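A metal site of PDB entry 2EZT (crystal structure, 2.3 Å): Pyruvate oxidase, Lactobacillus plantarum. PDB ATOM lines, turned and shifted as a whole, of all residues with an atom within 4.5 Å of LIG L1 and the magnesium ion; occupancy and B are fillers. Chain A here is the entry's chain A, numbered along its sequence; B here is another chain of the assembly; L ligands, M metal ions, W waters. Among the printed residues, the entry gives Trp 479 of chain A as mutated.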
ATOM      1  N   ASN A  92       2.880 -21.987 -12.565  1.00  0.00           N
ATOM      2  CA  ASN A  92       2.699 -22.330 -11.152  1.00  0.00           C
ATOM      3  C   ASN A  92       2.035 -21.242 -10.387  1.00  0.00           C
ATOM      4  O   ASN A  92       1.267 -21.507  -9.442  1.00  0.00           O
ATOM      5  CB  ASN A  92       4.009 -22.727 -10.454  1.00  0.00           C
ATOM      6  CG  ASN A  92       4.345 -24.178 -10.669  1.00  0.00           C
ATOM      7  OD1 ASN A  92       4.384 -24.648 -11.816  1.00  0.00           O
ATOM      8  ND2 ASN A  92       4.581 -24.913  -9.581  1.00  0.00           N
ATOM      9  N   VAL A 394       5.713 -23.715   1.362  1.00  0.00           N
ATOM     10  CA  VAL A 394       4.947 -24.955   1.413  1.00  0.00           C
ATOM     11  C   VAL A 394       5.846 -26.081   1.972  1.00  0.00           C
ATOM     12  O   VAL A 394       6.941 -26.288   1.486  1.00  0.00           O
ATOM     13  CB  VAL A 394       4.395 -25.302   0.009  1.00  0.00           C
ATOM     14  CG1 VAL A 394       3.853 -26.732  -0.052  1.00  0.00           C
ATOM     15  CG2 VAL A 394       3.317 -24.299  -0.403  1.00  0.00           C
ATOM     16  N   GLY A 395       5.366 -26.779   2.999  1.00  0.00           N
ATOM     17  CA  GLY A 395       6.095 -27.879   3.633  1.00  0.00           C
ATOM     18  C   GLY A 395       5.846 -27.851   5.131  1.00  0.00           C
ATOM     19  O   GLY A 395       4.800 -27.388   5.584  1.00  0.00           O
ATOM     20  N   ASP A 396       6.820 -28.342   5.917  1.00  0.00           N
ATOM     21  CA  ASP A 396       6.697 -28.300   7.389  1.00  0.00           C
ATOM     22  C   ASP A 396       6.322 -26.936   7.953  1.00  0.00           C
ATOM     23  O   ASP A 396       5.637 -26.859   8.977  1.00  0.00           O
ATOM     24  CB  ASP A 396       7.967 -28.785   8.061  1.00  0.00           C
ATOM     25  CG  ASP A 396       8.044 -30.277   8.183  1.00  0.00           C
ATOM     26  OD1 ASP A 396       7.028 -30.961   7.920  1.00  0.00           O
ATOM     27  OD2 ASP A 396       9.135 -30.769   8.528  1.00  0.00           O
ATOM     28  N   ILE A 397       6.754 -25.865   7.267  1.00  0.00           N
ATOM     29  CA  ILE A 397       6.531 -24.493   7.709  1.00  0.00           C
ATOM     30  C   ILE A 397       5.065 -24.128   7.850  1.00  0.00           C
ATOM     31  O   ILE A 397       4.717 -23.336   8.738  1.00  0.00           O
ATOM     32  CB  ILE A 397       7.255 -23.408   6.798  1.00  0.00           C
ATOM     33  CG1 ILE A 397       7.166 -22.001   7.436  1.00  0.00           C
ATOM     34  CG2 ILE A 397       6.682 -23.388   5.354  1.00  0.00           C
ATOM     35  CD1 ILE A 397       7.848 -21.868   8.825  1.00  0.00           C
ATOM     36  N   ALA A 420      -0.937 -25.393  -3.599  1.00  0.00           N
ATOM     37  CA  ALA A 420       0.198 -25.681  -2.707  1.00  0.00           C
ATOM     38  C   ALA A 420       1.542 -25.786  -3.454  1.00  0.00           C
ATOM     39  O   ALA A 420       2.316 -26.727  -3.271  1.00  0.00           O
ATOM     40  CB  ALA A 420      -0.063 -26.950  -1.840  1.00  0.00           C
ATOM     41  N   THR A 421       1.813 -24.784  -4.295  1.00  0.00           N
ATOM     42  CA  THR A 421       3.107 -24.717  -4.959  1.00  0.00           C
ATOM     43  C   THR A 421       4.203 -24.161  -4.053  1.00  0.00           C
ATOM     44  O   THR A 421       4.090 -23.072  -3.464  1.00  0.00           O
ATOM     45  CB  THR A 421       3.046 -23.912  -6.310  1.00  0.00           C
ATOM     46  OG1 THR A 421       4.337 -23.910  -6.916  1.00  0.00           O
ATOM     47  CG2 THR A 421       2.592 -22.432  -6.099  1.00  0.00           C
ATOM     48  N   MET A 422       5.288 -24.922  -3.961  1.00  0.00           N
ATOM     49  CA  MET A 422       6.516 -24.472  -3.318  1.00  0.00           C
ATOM     50  C   MET A 422       7.084 -23.267  -4.033  1.00  0.00           C
ATOM     51  O   MET A 422       6.899 -23.106  -5.251  1.00  0.00           O
ATOM     52  CB  MET A 422       7.556 -25.591  -3.299  1.00  0.00           C
ATOM     53  CG  MET A 422       7.287 -26.679  -2.285  1.00  0.00           C
ATOM     54  SD  MET A 422       8.255 -28.137  -2.686  1.00  0.00           S
ATOM     55  CE  MET A 422       9.894 -27.552  -2.263  1.00  0.00           C
ATOM     56  N   GLY A 446      10.822 -23.267   3.883  1.00  0.00           N
ATOM     57  CA  GLY A 446      11.742 -24.398   3.959  1.00  0.00           C
ATOM     58  C   GLY A 446      12.852 -24.229   2.939  1.00  0.00           C
ATOM     59  O   GLY A 446      12.749 -23.401   1.998  1.00  0.00           O
ATOM     60  N   ASP A 447      13.924 -25.009   3.116  1.00  0.00           N
ATOM     61  CA  ASP A 447      15.039 -24.934   2.175  1.00  0.00           C
ATOM     62  C   ASP A 447      14.706 -25.412   0.748  1.00  0.00           C
ATOM     63  O   ASP A 447      15.213 -24.834  -0.221  1.00  0.00           O
ATOM     64  CB  ASP A 447      16.326 -25.568   2.725  1.00  0.00           C
ATOM     65  CG  ASP A 447      16.155 -26.989   3.229  1.00  0.00           C
ATOM     66  OD1 ASP A 447      15.046 -27.551   3.216  1.00  0.00           O
ATOM     67  OD2 ASP A 447      17.169 -27.556   3.670  1.00  0.00           O
ATOM     68  N   GLY A 448      13.852 -26.424   0.610  1.00  0.00           N
ATOM     69  CA  GLY A 448      13.406 -26.889  -0.688  1.00  0.00           C
ATOM     70  C   GLY A 448      12.630 -25.837  -1.453  1.00  0.00           C
ATOM     71  O   GLY A 448      12.890 -25.601  -2.648  1.00  0.00           O
ATOM     72  N   GLY A 449      11.655 -25.222  -0.787  1.00  0.00           N
ATOM     73  CA  GLY A 449      10.883 -24.138  -1.386  1.00  0.00           C
ATOM     74  C   GLY A 449      11.643 -22.846  -1.624  1.00  0.00           C
ATOM     75  O   GLY A 449      11.490 -22.229  -2.667  1.00  0.00           O
ATOM     76  N   MET A 452      13.699 -23.093  -4.859  1.00  0.00           N
ATOM     77  CA  MET A 452      13.031 -23.026  -6.143  1.00  0.00           C
ATOM     78  C   MET A 452      12.962 -21.605  -6.697  1.00  0.00           C
ATOM     79  O   MET A 452      13.039 -21.431  -7.923  1.00  0.00           O
ATOM     80  CB  MET A 452      11.657 -23.668  -6.053  1.00  0.00           C
ATOM     81  CG  MET A 452      11.771 -25.174  -5.847  1.00  0.00           C
ATOM     82  SD  MET A 452      10.168 -25.925  -5.919  1.00  0.00           S
ATOM     83  CE  MET A 452      10.583 -27.686  -5.967  1.00  0.00           C
ATOM     84  N   PHE A 472      14.305 -22.386   6.679  1.00  0.00           N
ATOM     85  CA  PHE A 472      14.371 -23.506   7.634  1.00  0.00           C
ATOM     86  C   PHE A 472      15.138 -24.656   6.987  1.00  0.00           C
ATOM     87  O   PHE A 472      14.564 -25.458   6.263  1.00  0.00           O
ATOM     88  CB  PHE A 472      12.963 -23.938   8.087  1.00  0.00           C
ATOM     89  CG  PHE A 472      12.238 -22.876   8.884  1.00  0.00           C
ATOM     90  CD1 PHE A 472      11.768 -21.707   8.255  1.00  0.00           C
ATOM     91  CD2 PHE A 472      12.055 -23.030  10.260  1.00  0.00           C
ATOM     92  CE1 PHE A 472      11.137 -20.694   9.008  1.00  0.00           C
ATOM     93  CE2 PHE A 472      11.382 -22.043  11.016  1.00  0.00           C
ATOM     94  CZ  PHE A 472      10.932 -20.863  10.389  1.00  0.00           C
ATOM     95  N   ASN A 474      16.716 -27.934   6.838  1.00  0.00           N
ATOM     96  CA  ASN A 474      16.814 -29.280   7.405  1.00  0.00           C
ATOM     97  C   ASN A 474      17.527 -30.266   6.473  1.00  0.00           C
ATOM     98  O   ASN A 474      17.751 -31.426   6.849  1.00  0.00           O
ATOM     99  CB  ASN A 474      15.416 -29.802   7.850  1.00  0.00           C
ATOM    100  CG  ASN A 474      14.387 -29.701   6.758  1.00  0.00           C
ATOM    101  OD1 ASN A 474      14.717 -29.385   5.622  1.00  0.00           O
ATOM    102  ND2 ASN A 474      13.138 -29.959   7.089  1.00  0.00           N
ATOM    103  N   GLN A 476      16.288 -31.521   3.850  1.00  0.00           N
ATOM    104  CA  GLN A 476      15.272 -32.512   3.516  1.00  0.00           C
ATOM    105  C   GLN A 476      14.098 -31.808   2.908  1.00  0.00           C
ATOM    106  O   GLN A 476      13.921 -30.611   3.067  1.00  0.00           O
ATOM    107  CB  GLN A 476      14.766 -33.269   4.761  1.00  0.00           C
ATOM    108  CG  GLN A 476      15.823 -33.846   5.691  1.00  0.00           C
ATOM    109  CD  GLN A 476      15.259 -34.304   7.027  1.00  0.00           C
ATOM    110  OE1 GLN A 476      15.894 -35.059   7.744  1.00  0.00           O
ATOM    111  NE2 GLN A 476      14.055 -33.856   7.350  1.00  0.00           N
ATOM    112  N   TYR A 477      13.298 -32.581   2.172  1.00  0.00           N
ATOM    113  CA  TYR A 477      11.909 -32.258   1.969  1.00  0.00           C
ATOM    114  C   TYR A 477      11.212 -32.964   3.142  1.00  0.00           C
ATOM    115  O   TYR A 477      10.774 -34.127   3.014  1.00  0.00           O
ATOM    116  CB  TYR A 477      11.456 -32.848   0.632  1.00  0.00           C
ATOM    117  CG  TYR A 477      12.129 -32.235  -0.589  1.00  0.00           C
ATOM    118  CD1 TYR A 477      12.097 -30.837  -0.809  1.00  0.00           C
ATOM    119  CD2 TYR A 477      12.768 -33.034  -1.539  1.00  0.00           C
ATOM    120  CE1 TYR A 477      12.708 -30.262  -1.915  1.00  0.00           C
ATOM    121  CE2 TYR A 477      13.380 -32.469  -2.679  1.00  0.00           C
ATOM    122  CZ  TYR A 477      13.357 -31.071  -2.855  1.00  0.00           C
ATOM    123  OH  TYR A 477      13.961 -30.512  -3.963  1.00  0.00           O
ATOM    124  N   GLY A 478      11.156 -32.307   4.294  1.00  0.00           N
ATOM    125  CA  GLY A 478      10.740 -32.981   5.532  1.00  0.00           C
ATOM    126  C   GLY A 478       9.306 -33.482   5.436  1.00  0.00           C
ATOM    127  O   GLY A 478       9.007 -34.637   5.810  1.00  0.00           O
ATOM    128  N   TRP A 479       8.428 -32.609   4.916  1.00  0.00           N
ATOM    129  CA  TRP A 479       7.027 -32.927   4.677  1.00  0.00           C
ATOM    130  C   TRP A 479       6.863 -34.251   3.948  1.00  0.00           C
ATOM    131  O   TRP A 479       6.050 -35.089   4.361  1.00  0.00           O
ATOM    132  CB  TRP A 479       6.381 -31.800   3.865  1.00  0.00           C
ATOM    133  CG  TRP A 479       4.858 -31.772   3.865  1.00  0.00           C
ATOM    134  CD1 TRP A 479       4.045 -32.093   2.844  1.00  0.00           C
ATOM    135  CD2 TRP A 479       3.990 -31.331   4.946  1.00  0.00           C
ATOM    136  NE1 TRP A 479       2.728 -31.912   3.191  1.00  0.00           N
ATOM    137  CE2 TRP A 479       2.670 -31.424   4.471  1.00  0.00           C
ATOM    138  CE3 TRP A 479       4.211 -30.869   6.249  1.00  0.00           C
ATOM    139  CZ2 TRP A 479       1.544 -31.092   5.263  1.00  0.00           C
ATOM    140  CZ3 TRP A 479       3.101 -30.533   7.051  1.00  0.00           C
ATOM    141  CH2 TRP A 479       1.786 -30.644   6.540  1.00  0.00           C
ATOM    142  N   ILE A 480       7.654 -34.443   2.878  1.00  0.00           N
ATOM    143  CA  ILE A 480       7.620 -35.670   2.053  1.00  0.00           C
ATOM    144  C   ILE A 480       8.381 -36.869   2.670  1.00  0.00           C
ATOM    145  O   ILE A 480       7.984 -38.039   2.503  1.00  0.00           O
ATOM    146  CB  ILE A 480       8.160 -35.383   0.614  1.00  0.00           C
ATOM    147  CG1 ILE A 480       7.468 -34.163   0.014  1.00  0.00           C
ATOM    148  CG2 ILE A 480       7.994 -36.621  -0.288  1.00  0.00           C
ATOM    149  CD1 ILE A 480       5.947 -34.220   0.072  1.00  0.00           C
ATOM    150  N   ILE B  32      11.310 -34.730  -8.389  1.00  0.00           N
ATOM    151  CA  ILE B  32      11.186 -34.391  -6.971  1.00  0.00           C
ATOM    152  C   ILE B  32      10.013 -35.174  -6.416  1.00  0.00           C
ATOM    153  O   ILE B  32       8.953 -35.202  -7.018  1.00  0.00           O
ATOM    154  CB  ILE B  32      10.976 -32.847  -6.766  1.00  0.00           C
ATOM    155  CG1 ILE B  32      12.254 -32.097  -7.182  1.00  0.00           C
ATOM    156  CG2 ILE B  32      10.489 -32.506  -5.346  1.00  0.00           C
ATOM    157  CD1 ILE B  32      12.189 -30.625  -7.068  1.00  0.00           C
ATOM    158  N   PRO B  33      10.211 -35.848  -5.263  1.00  0.00           N
ATOM    159  CA  PRO B  33       9.117 -36.681  -4.709  1.00  0.00           C
ATOM    160  C   PRO B  33       7.969 -35.859  -4.129  1.00  0.00           C
ATOM    161  O   PRO B  33       8.148 -34.692  -3.799  1.00  0.00           O
ATOM    162  CB  PRO B  33       9.807 -37.464  -3.589  1.00  0.00           C
ATOM    163  CG  PRO B  33      10.924 -36.574  -3.166  1.00  0.00           C
ATOM    164  CD  PRO B  33      11.404 -35.852  -4.395  1.00  0.00           C
ATOM    165  N   GLY B  34       6.795 -36.483  -4.032  1.00  0.00           N
ATOM    166  CA  GLY B  34       5.686 -35.970  -3.262  1.00  0.00           C
ATOM    167  C   GLY B  34       4.810 -37.147  -2.904  1.00  0.00           C
ATOM    168  O   GLY B  34       4.983 -38.222  -3.497  1.00  0.00           O
ATOM    169  N   GLU B  59      11.653 -28.953 -10.589  1.00  0.00           N
ATOM    170  CA  GLU B  59      11.228 -29.929 -11.626  1.00  0.00           C
ATOM    171  C   GLU B  59      11.502 -29.503 -13.070  1.00  0.00           C
ATOM    172  O   GLU B  59      11.639 -30.380 -13.915  1.00  0.00           O
ATOM    173  CB  GLU B  59       9.767 -30.422 -11.458  1.00  0.00           C
ATOM    174  CG  GLU B  59       9.460 -31.043 -10.072  1.00  0.00           C
ATOM    175  CD  GLU B  59       9.087 -29.990  -9.013  1.00  0.00           C
ATOM    176  OE1 GLU B  59       9.350 -28.763  -9.199  1.00  0.00           O
ATOM    177  OE2 GLU B  59       8.509 -30.400  -7.984  1.00  0.00           O
ATOM    178  N   SER B  82       5.356 -34.319  -9.054  1.00  0.00           N
ATOM    179  CA  SER B  82       4.213 -34.669  -8.213  1.00  0.00           C
ATOM    180  C   SER B  82       2.947 -33.912  -8.669  1.00  0.00           C
ATOM    181  O   SER B  82       3.005 -32.993  -9.504  1.00  0.00           O
ATOM    182  CB  SER B  82       4.537 -34.333  -6.759  1.00  0.00           C
ATOM    183  OG  SER B  82       5.071 -33.018  -6.703  1.00  0.00           O
ATOM    184  N   PRO B  85       1.586 -28.604  -8.776  1.00  0.00           N
ATOM    185  CA  PRO B  85       2.805 -27.786  -9.003  1.00  0.00           C
ATOM    186  C   PRO B  85       4.065 -28.543  -9.426  1.00  0.00           C
ATOM    187  O   PRO B  85       4.904 -27.998 -10.108  1.00  0.00           O
ATOM    188  CB  PRO B  85       3.016 -27.118  -7.639  1.00  0.00           C
ATOM    189  CG  PRO B  85       2.329 -27.966  -6.676  1.00  0.00           C
ATOM    190  CD  PRO B  85       1.102 -28.443  -7.402  1.00  0.00           C
ATOM    191  N   GLY B  86       4.198 -29.805  -9.031  1.00  0.00           N
ATOM    192  CA  GLY B  86       5.357 -30.616  -9.444  1.00  0.00           C
ATOM    193  C   GLY B  86       5.414 -30.773 -10.946  1.00  0.00           C
ATOM    194  O   GLY B  86       6.439 -30.487 -11.573  1.00  0.00           O
ATOM    195  N   HIS B  89       5.647 -27.471 -13.151  1.00  0.00           N
ATOM    196  CA  HIS B  89       7.053 -27.043 -13.220  1.00  0.00           C
ATOM    197  C   HIS B  89       7.829 -27.678 -14.385  1.00  0.00           C
ATOM    198  O   HIS B  89       8.827 -27.113 -14.830  1.00  0.00           O
ATOM    199  CB  HIS B  89       7.802 -27.356 -11.917  1.00  0.00           C
ATOM    200  CG  HIS B  89       7.900 -26.193 -10.968  1.00  0.00           C
ATOM    201  ND1 HIS B  89       8.419 -26.330  -9.706  1.00  0.00           N
ATOM    202  CD2 HIS B  89       7.543 -24.894 -11.098  1.00  0.00           C
ATOM    203  CE1 HIS B  89       8.416 -25.156  -9.101  1.00  0.00           C
ATOM    204  NE2 HIS B  89       7.879 -24.272  -9.918  1.00  0.00           N
ATOM    205  N   PHE B 121      -7.082 -31.984  -1.584  1.00  0.00           N
ATOM    206  CA  PHE B 121      -5.895 -31.155  -1.560  1.00  0.00           C
ATOM    207  C   PHE B 121      -4.996 -31.395  -2.772  1.00  0.00           C
ATOM    208  O   PHE B 121      -4.638 -32.543  -3.078  1.00  0.00           O
ATOM    209  CB  PHE B 121      -5.155 -31.458  -0.266  1.00  0.00           C
ATOM    210  CG  PHE B 121      -3.837 -30.792  -0.170  1.00  0.00           C
ATOM    211  CD1 PHE B 121      -3.748 -29.443   0.131  1.00  0.00           C
ATOM    212  CD2 PHE B 121      -2.672 -31.499  -0.380  1.00  0.00           C
ATOM    213  CE1 PHE B 121      -2.525 -28.820   0.222  1.00  0.00           C
ATOM    214  CE2 PHE B 121      -1.448 -30.876  -0.289  1.00  0.00           C
ATOM    215  CZ  PHE B 121      -1.369 -29.543   0.035  1.00  0.00           C
ATOM    216  N   GLN B 122      -4.648 -30.313  -3.486  1.00  0.00           N
ATOM    217  CA  GLN B 122      -3.761 -30.400  -4.662  1.00  0.00           C
ATOM    218  C   GLN B 122      -4.321 -31.376  -5.718  1.00  0.00           C
ATOM    219  O   GLN B 122      -3.576 -31.913  -6.545  1.00  0.00           O
ATOM    220  CB  GLN B 122      -2.371 -30.863  -4.220  1.00  0.00           C
ATOM    221  CG  GLN B 122      -1.190 -30.252  -4.890  1.00  0.00           C
ATOM    222  CD  GLN B 122       0.073 -30.366  -4.016  1.00  0.00           C
ATOM    223  OE1 GLN B 122       0.261 -31.356  -3.332  1.00  0.00           O
ATOM    224  NE2 GLN B 122       0.902 -29.352  -4.030  1.00  0.00           N
HETATM  225  O1  LIG L   1      12.338 -28.148   2.405  1.00  0.00           O
HETATM  226  P1  LIG L   1      10.859 -27.948   2.156  1.00  0.00           P
HETATM  227  O2  LIG L   1      10.435 -26.677   1.500  1.00  0.00           O
HETATM  228  O3  LIG L   1      10.099 -27.995   3.564  1.00  0.00           O
HETATM  229  P2  LIG L   1      10.356 -28.859   4.894  1.00  0.00           P
HETATM  230  O4  LIG L   1      10.359 -27.779   5.990  1.00  0.00           O
HETATM  231  O5  LIG L   1      11.687 -29.596   4.786  1.00  0.00           O
HETATM  232  O6  LIG L   1       9.107 -29.709   4.918  1.00  0.00           O
HETATM  233  O7  LIG L   1      10.225 -29.133   1.336  1.00  0.00           O
HETATM  234  C1  LIG L   1       8.827 -29.116   1.019  1.00  0.00           C
HETATM  235  C2  LIG L   1       8.531 -30.551   0.622  1.00  0.00           C
HETATM  236  C3  LIG L   1       7.297 -30.704  -0.257  1.00  0.00           C
HETATM  237  S1  LIG L   1       5.767 -30.255   0.469  1.00  0.00           S
HETATM  238  C4  LIG L   1       4.925 -30.748  -1.006  1.00  0.00           C
HETATM  239  C5  LIG L   1       3.427 -30.607  -0.969  1.00  0.00           C
HETATM  240  C6  LIG L   1       2.724 -30.092   0.259  1.00  0.00           C
HETATM  241  O8  LIG L   1       2.648 -30.896  -2.018  1.00  0.00           O
HETATM  242  N1  LIG L   1       5.806 -31.176  -1.982  1.00  0.00           N
HETATM  243  C7  LIG L   1       7.121 -31.157  -1.574  1.00  0.00           C
HETATM  244  C8  LIG L   1       8.283 -31.612  -2.435  1.00  0.00           C
HETATM  245  C9  LIG L   1       5.414 -31.589  -3.351  1.00  0.00           C
HETATM  246  C10 LIG L   1       5.731 -30.400  -4.300  1.00  0.00           C
HETATM  247  C11 LIG L   1       5.026 -29.176  -4.258  1.00  0.00           C
HETATM  248  N2  LIG L   1       4.015 -28.933  -3.388  1.00  0.00           N
HETATM  249  N3  LIG L   1       5.354 -28.177  -5.128  1.00  0.00           N
HETATM  250  C12 LIG L   1       6.343 -28.340  -6.042  1.00  0.00           C
HETATM  251  C13 LIG L   1       6.666 -27.199  -6.958  1.00  0.00           C
HETATM  252  N4  LIG L   1       7.040 -29.496  -6.106  1.00  0.00           N
HETATM  253  C14 LIG L   1       6.747 -30.514  -5.260  1.00  0.00           C
HETATM  254  P1  LG2 L   2     -11.447 -21.780   0.592  1.00  0.00           P
HETATM  255  O1  LG2 L   2     -10.960 -20.553  -0.143  1.00  0.00           O
HETATM  256  O2  LG2 L   2     -11.244 -23.133  -0.038  1.00  0.00           O
HETATM  257  O3  LG2 L   2     -13.013 -21.591   0.916  1.00  0.00           O
HETATM  258  C1  LG2 L   2     -13.596 -20.350   1.293  1.00  0.00           C
HETATM  259  C2  LG2 L   2     -15.090 -20.615   1.321  1.00  0.00           C
HETATM  260  O4  LG2 L   2     -15.779 -19.470   1.832  1.00  0.00           O
HETATM  261  C3  LG2 L   2     -15.680 -20.879  -0.068  1.00  0.00           C
HETATM  262  O5  LG2 L   2     -16.547 -22.008   0.044  1.00  0.00           O
HETATM  263  C4  LG2 L   2     -16.454 -19.598  -0.402  1.00  0.00           C
HETATM  264  O6  LG2 L   2     -17.582 -19.816  -1.241  1.00  0.00           O
HETATM  265  C5  LG2 L   2     -16.884 -19.153   0.973  1.00  0.00           C
HETATM  266  N1  LG2 L   2     -17.104 -17.686   1.081  1.00  0.00           N
HETATM  267  C6  LG2 L   2     -16.375 -16.712   0.520  1.00  0.00           C
HETATM  268  N2  LG2 L   2     -16.871 -15.518   0.902  1.00  0.00           N
HETATM  269  C7  LG2 L   2     -17.939 -15.748   1.717  1.00  0.00           C
HETATM  270  C8  LG2 L   2     -18.841 -14.927   2.414  1.00  0.00           C
HETATM  271  N3  LG2 L   2     -18.784 -13.561   2.340  1.00  0.00           N
HETATM  272  N4  LG2 L   2     -19.801 -15.515   3.170  1.00  0.00           N
HETATM  273  C9  LG2 L   2     -19.897 -16.859   3.255  1.00  0.00           C
HETATM  274  N5  LG2 L   2     -19.035 -17.672   2.598  1.00  0.00           N
HETATM  275  C10 LG2 L   2     -18.066 -17.138   1.835  1.00  0.00           C
HETATM  276  N6  LG2 L   2      -5.773 -26.759   5.646  1.00  0.00           N
HETATM  277  C11 LG2 L   2      -6.245 -27.323   6.781  1.00  0.00           C
HETATM  278  O7  LG2 L   2      -7.186 -26.770   7.406  1.00  0.00           O
HETATM  279  N7  LG2 L   2      -5.699 -28.482   7.232  1.00  0.00           N
HETATM  280  C12 LG2 L   2      -4.683 -29.094   6.559  1.00  0.00           C
HETATM  281  O8  LG2 L   2      -4.197 -30.159   6.998  1.00  0.00           O
HETATM  282  C13 LG2 L   2      -4.177 -28.511   5.401  1.00  0.00           C
HETATM  283  N8  LG2 L   2      -3.153 -29.067   4.668  1.00  0.00           N
HETATM  284  C14 LG2 L   2      -2.386 -28.177   3.922  1.00  0.00           C
HETATM  285  C15 LG2 L   2      -1.043 -28.433   3.612  1.00  0.00           C
HETATM  286  C16 LG2 L   2      -0.283 -27.516   2.882  1.00  0.00           C
HETATM  287  C17 LG2 L   2       1.162 -27.870   2.598  1.00  0.00           C
HETATM  288  C18 LG2 L   2      -0.869 -26.294   2.459  1.00  0.00           C
HETATM  289  C19 LG2 L   2      -0.104 -25.257   1.660  1.00  0.00           C
HETATM  290  C20 LG2 L   2      -2.207 -26.042   2.783  1.00  0.00           C
HETATM  291  C21 LG2 L   2      -2.970 -26.969   3.504  1.00  0.00           C
HETATM  292  N9  LG2 L   2      -4.284 -26.751   3.827  1.00  0.00           N
HETATM  293  C22 LG2 L   2      -4.743 -27.321   4.964  1.00  0.00           C
HETATM  294  C23 LG2 L   2      -4.968 -25.542   3.352  1.00  0.00           C
HETATM  295  C24 LG2 L   2      -6.091 -26.240   2.504  1.00  0.00           C
HETATM  296  O9  LG2 L   2      -5.606 -26.959   1.351  1.00  0.00           O
HETATM  297  C25 LG2 L   2      -7.312 -25.403   2.071  1.00  0.00           C
HETATM  298  O10 LG2 L   2      -6.920 -24.318   1.211  1.00  0.00           O
HETATM  299  C26 LG2 L   2      -8.140 -24.918   3.278  1.00  0.00           C
HETATM  300  O11 LG2 L   2      -8.302 -25.936   4.283  1.00  0.00           O
HETATM  301  C27 LG2 L   2      -9.524 -24.428   2.870  1.00  0.00           C
HETATM  302  O12 LG2 L   2      -9.759 -23.238   3.631  1.00  0.00           O
HETATM  303  P2  LG2 L   2     -11.049 -22.303   3.481  1.00  0.00           P
HETATM  304  O13 LG2 L   2     -12.298 -23.132   3.456  1.00  0.00           O
HETATM  305  O14 LG2 L   2     -10.841 -21.234   4.516  1.00  0.00           O
HETATM  306  O15 LG2 L   2     -10.707 -21.679   2.022  1.00  0.00           O
HETATM  307 MG    MG M   1      13.489 -28.711   4.017  1.00  0.00          MG
HETATM  308  O   HOH W   1      10.962 -26.984   8.603  1.00  0.00           O
HETATM  309  O   HOH W   2       8.929 -24.793   2.469  1.00  0.00           O
HETATM  310  O   HOH W   3       8.859 -25.771   5.166  1.00  0.00           O
HETATM  311  O   HOH W   4      12.862 -27.015   5.309  1.00  0.00           O
HETATM  312  O   HOH W   5       2.838 -31.627  -5.627  1.00  0.00           O
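N of Asp 396 sits at hydrogen-bond distance from O6 of LIG L1 (2.8 Å). O of Ala 420 sits at hydrogen-bond distance from N2 of LIG L1 (2.8 Å). N of Met 422 is in hydrogen-bond range of N3 of LIG L1, at 3.5 Å. The backbone NH (N) of Trp 479 lies within hydrogen-bond range of an oxygen (O6) of LIG L1 (3.0 Å). O8 of LIG L1 lies within hydrogen-bond range of OE1 of Gln 122 of chain B (2.8 Å). O6 of LIG L1 sits at hydrogen-bond distance from N of Gly 478, 3.4 Å away. N of Gly 448 sits close to O1 of LIG L1. A nitrogen (N4) of LIG L1 lies within hydrogen-bond range of the side-chain carboxylate (OE2) of Glu 59 of chain B, 2.5 Å away. The backbone NH (N) of Gly 449 is in hydrogen-bond range of an oxygen (O2) of LIG L1 (3.0 Å).
OE1 of Glu 59 of chain B lies within hydrogen-bond range of ND1 of His 89 of chain B (2.7 Å). The backbone carbonyl oxygen (O) of Pro 85 of chain B is in hydrogen-bond range of the side-chain amide nitrogen (ND2) of Asn 92. N of His 89 of chain B sits close to OD1 of Asn 92 (3.4 Å). The side-chain amide nitrogen (NE2) of Gln 122 of chain B lies within hydrogen-bond range of the backbone carbonyl oxygen (O) of Ala 420 (3.1 Å). The backbone NH of Asp 447 sits at hydrogen-bond distance from the backbone carbonyl oxygen of Phe 472, 3.2 Å away.
Val 394 touches LIG L1 (O to C1, 3.4 Å). Gly 395 touches LIG L1 (CA to O6, 3.8 Å). Gly 446 touches LIG L1. Met 452 touches LIG L1. Tyr 477 touches LIG L1 (CD1 to O7, 3.3 Å). Ile 480 touches LIG L1 (CG1 to C7, 3.4 Å). Ile 32 of chain B touches LIG L1. O of Pro 33 of chain B touches C8 of LIG L1, at 3.4 Å. OG of Ser 82 of chain B touches C14 of LIG L1 (3.3 Å). Pro 85 of chain B touches LIG L1 (CG to N3, 3.4 Å). Gly 86 of chain B touches LIG L1 (CA to N4, 3.9 Å). His 89 of chain B touches LIG L1. Hydrophobic or aromatic side chains that line LIG L1: Val 394, Met 422, Met 452, Tyr 477, Trp 479, Ile 480, Ile 32 of chain B, Pro 85 of chain B and His 89 of chain B.
Three residues have an atom within 4 Å of the magnesium ion: Asp 447, Asn 474 and Gln 476. The nearest printed residue that does not touch the magnesium ion is Phe 472 (4.1 Å).
The magnesium ion is bound by O1 of LIG L1 (2.1 Å), OD1 of Asp 447 (2.1 Å), OD1 of Asn 474 (2.1 Å), O5 of LIG L1 (2.1 Å), O of Gln 476 (2.2 Å) and water W4 (2.2 Å). The magnesium ion has six donor atoms within binding distance.
Water W4 lies within hydrogen-bond range of O of Phe 472 (2.5 Å), O4 of LIG L1 (2.7 Å), N of Asp 447 (3.2 Å) and ND2 of Asn 474 (3.5 Å). Water W2 lies within hydrogen-bond range of O2 of LIG L1 (2.6 Å), O of Val 394 (2.7 Å) and N of Gly 446 (2.8 Å). Water W5 bridges the side-chain hydroxyl of Ser 82 of chain B (2.8 Å) and the side-chain amide nitrogen of Gln 122 of chain B (3.4 Å).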
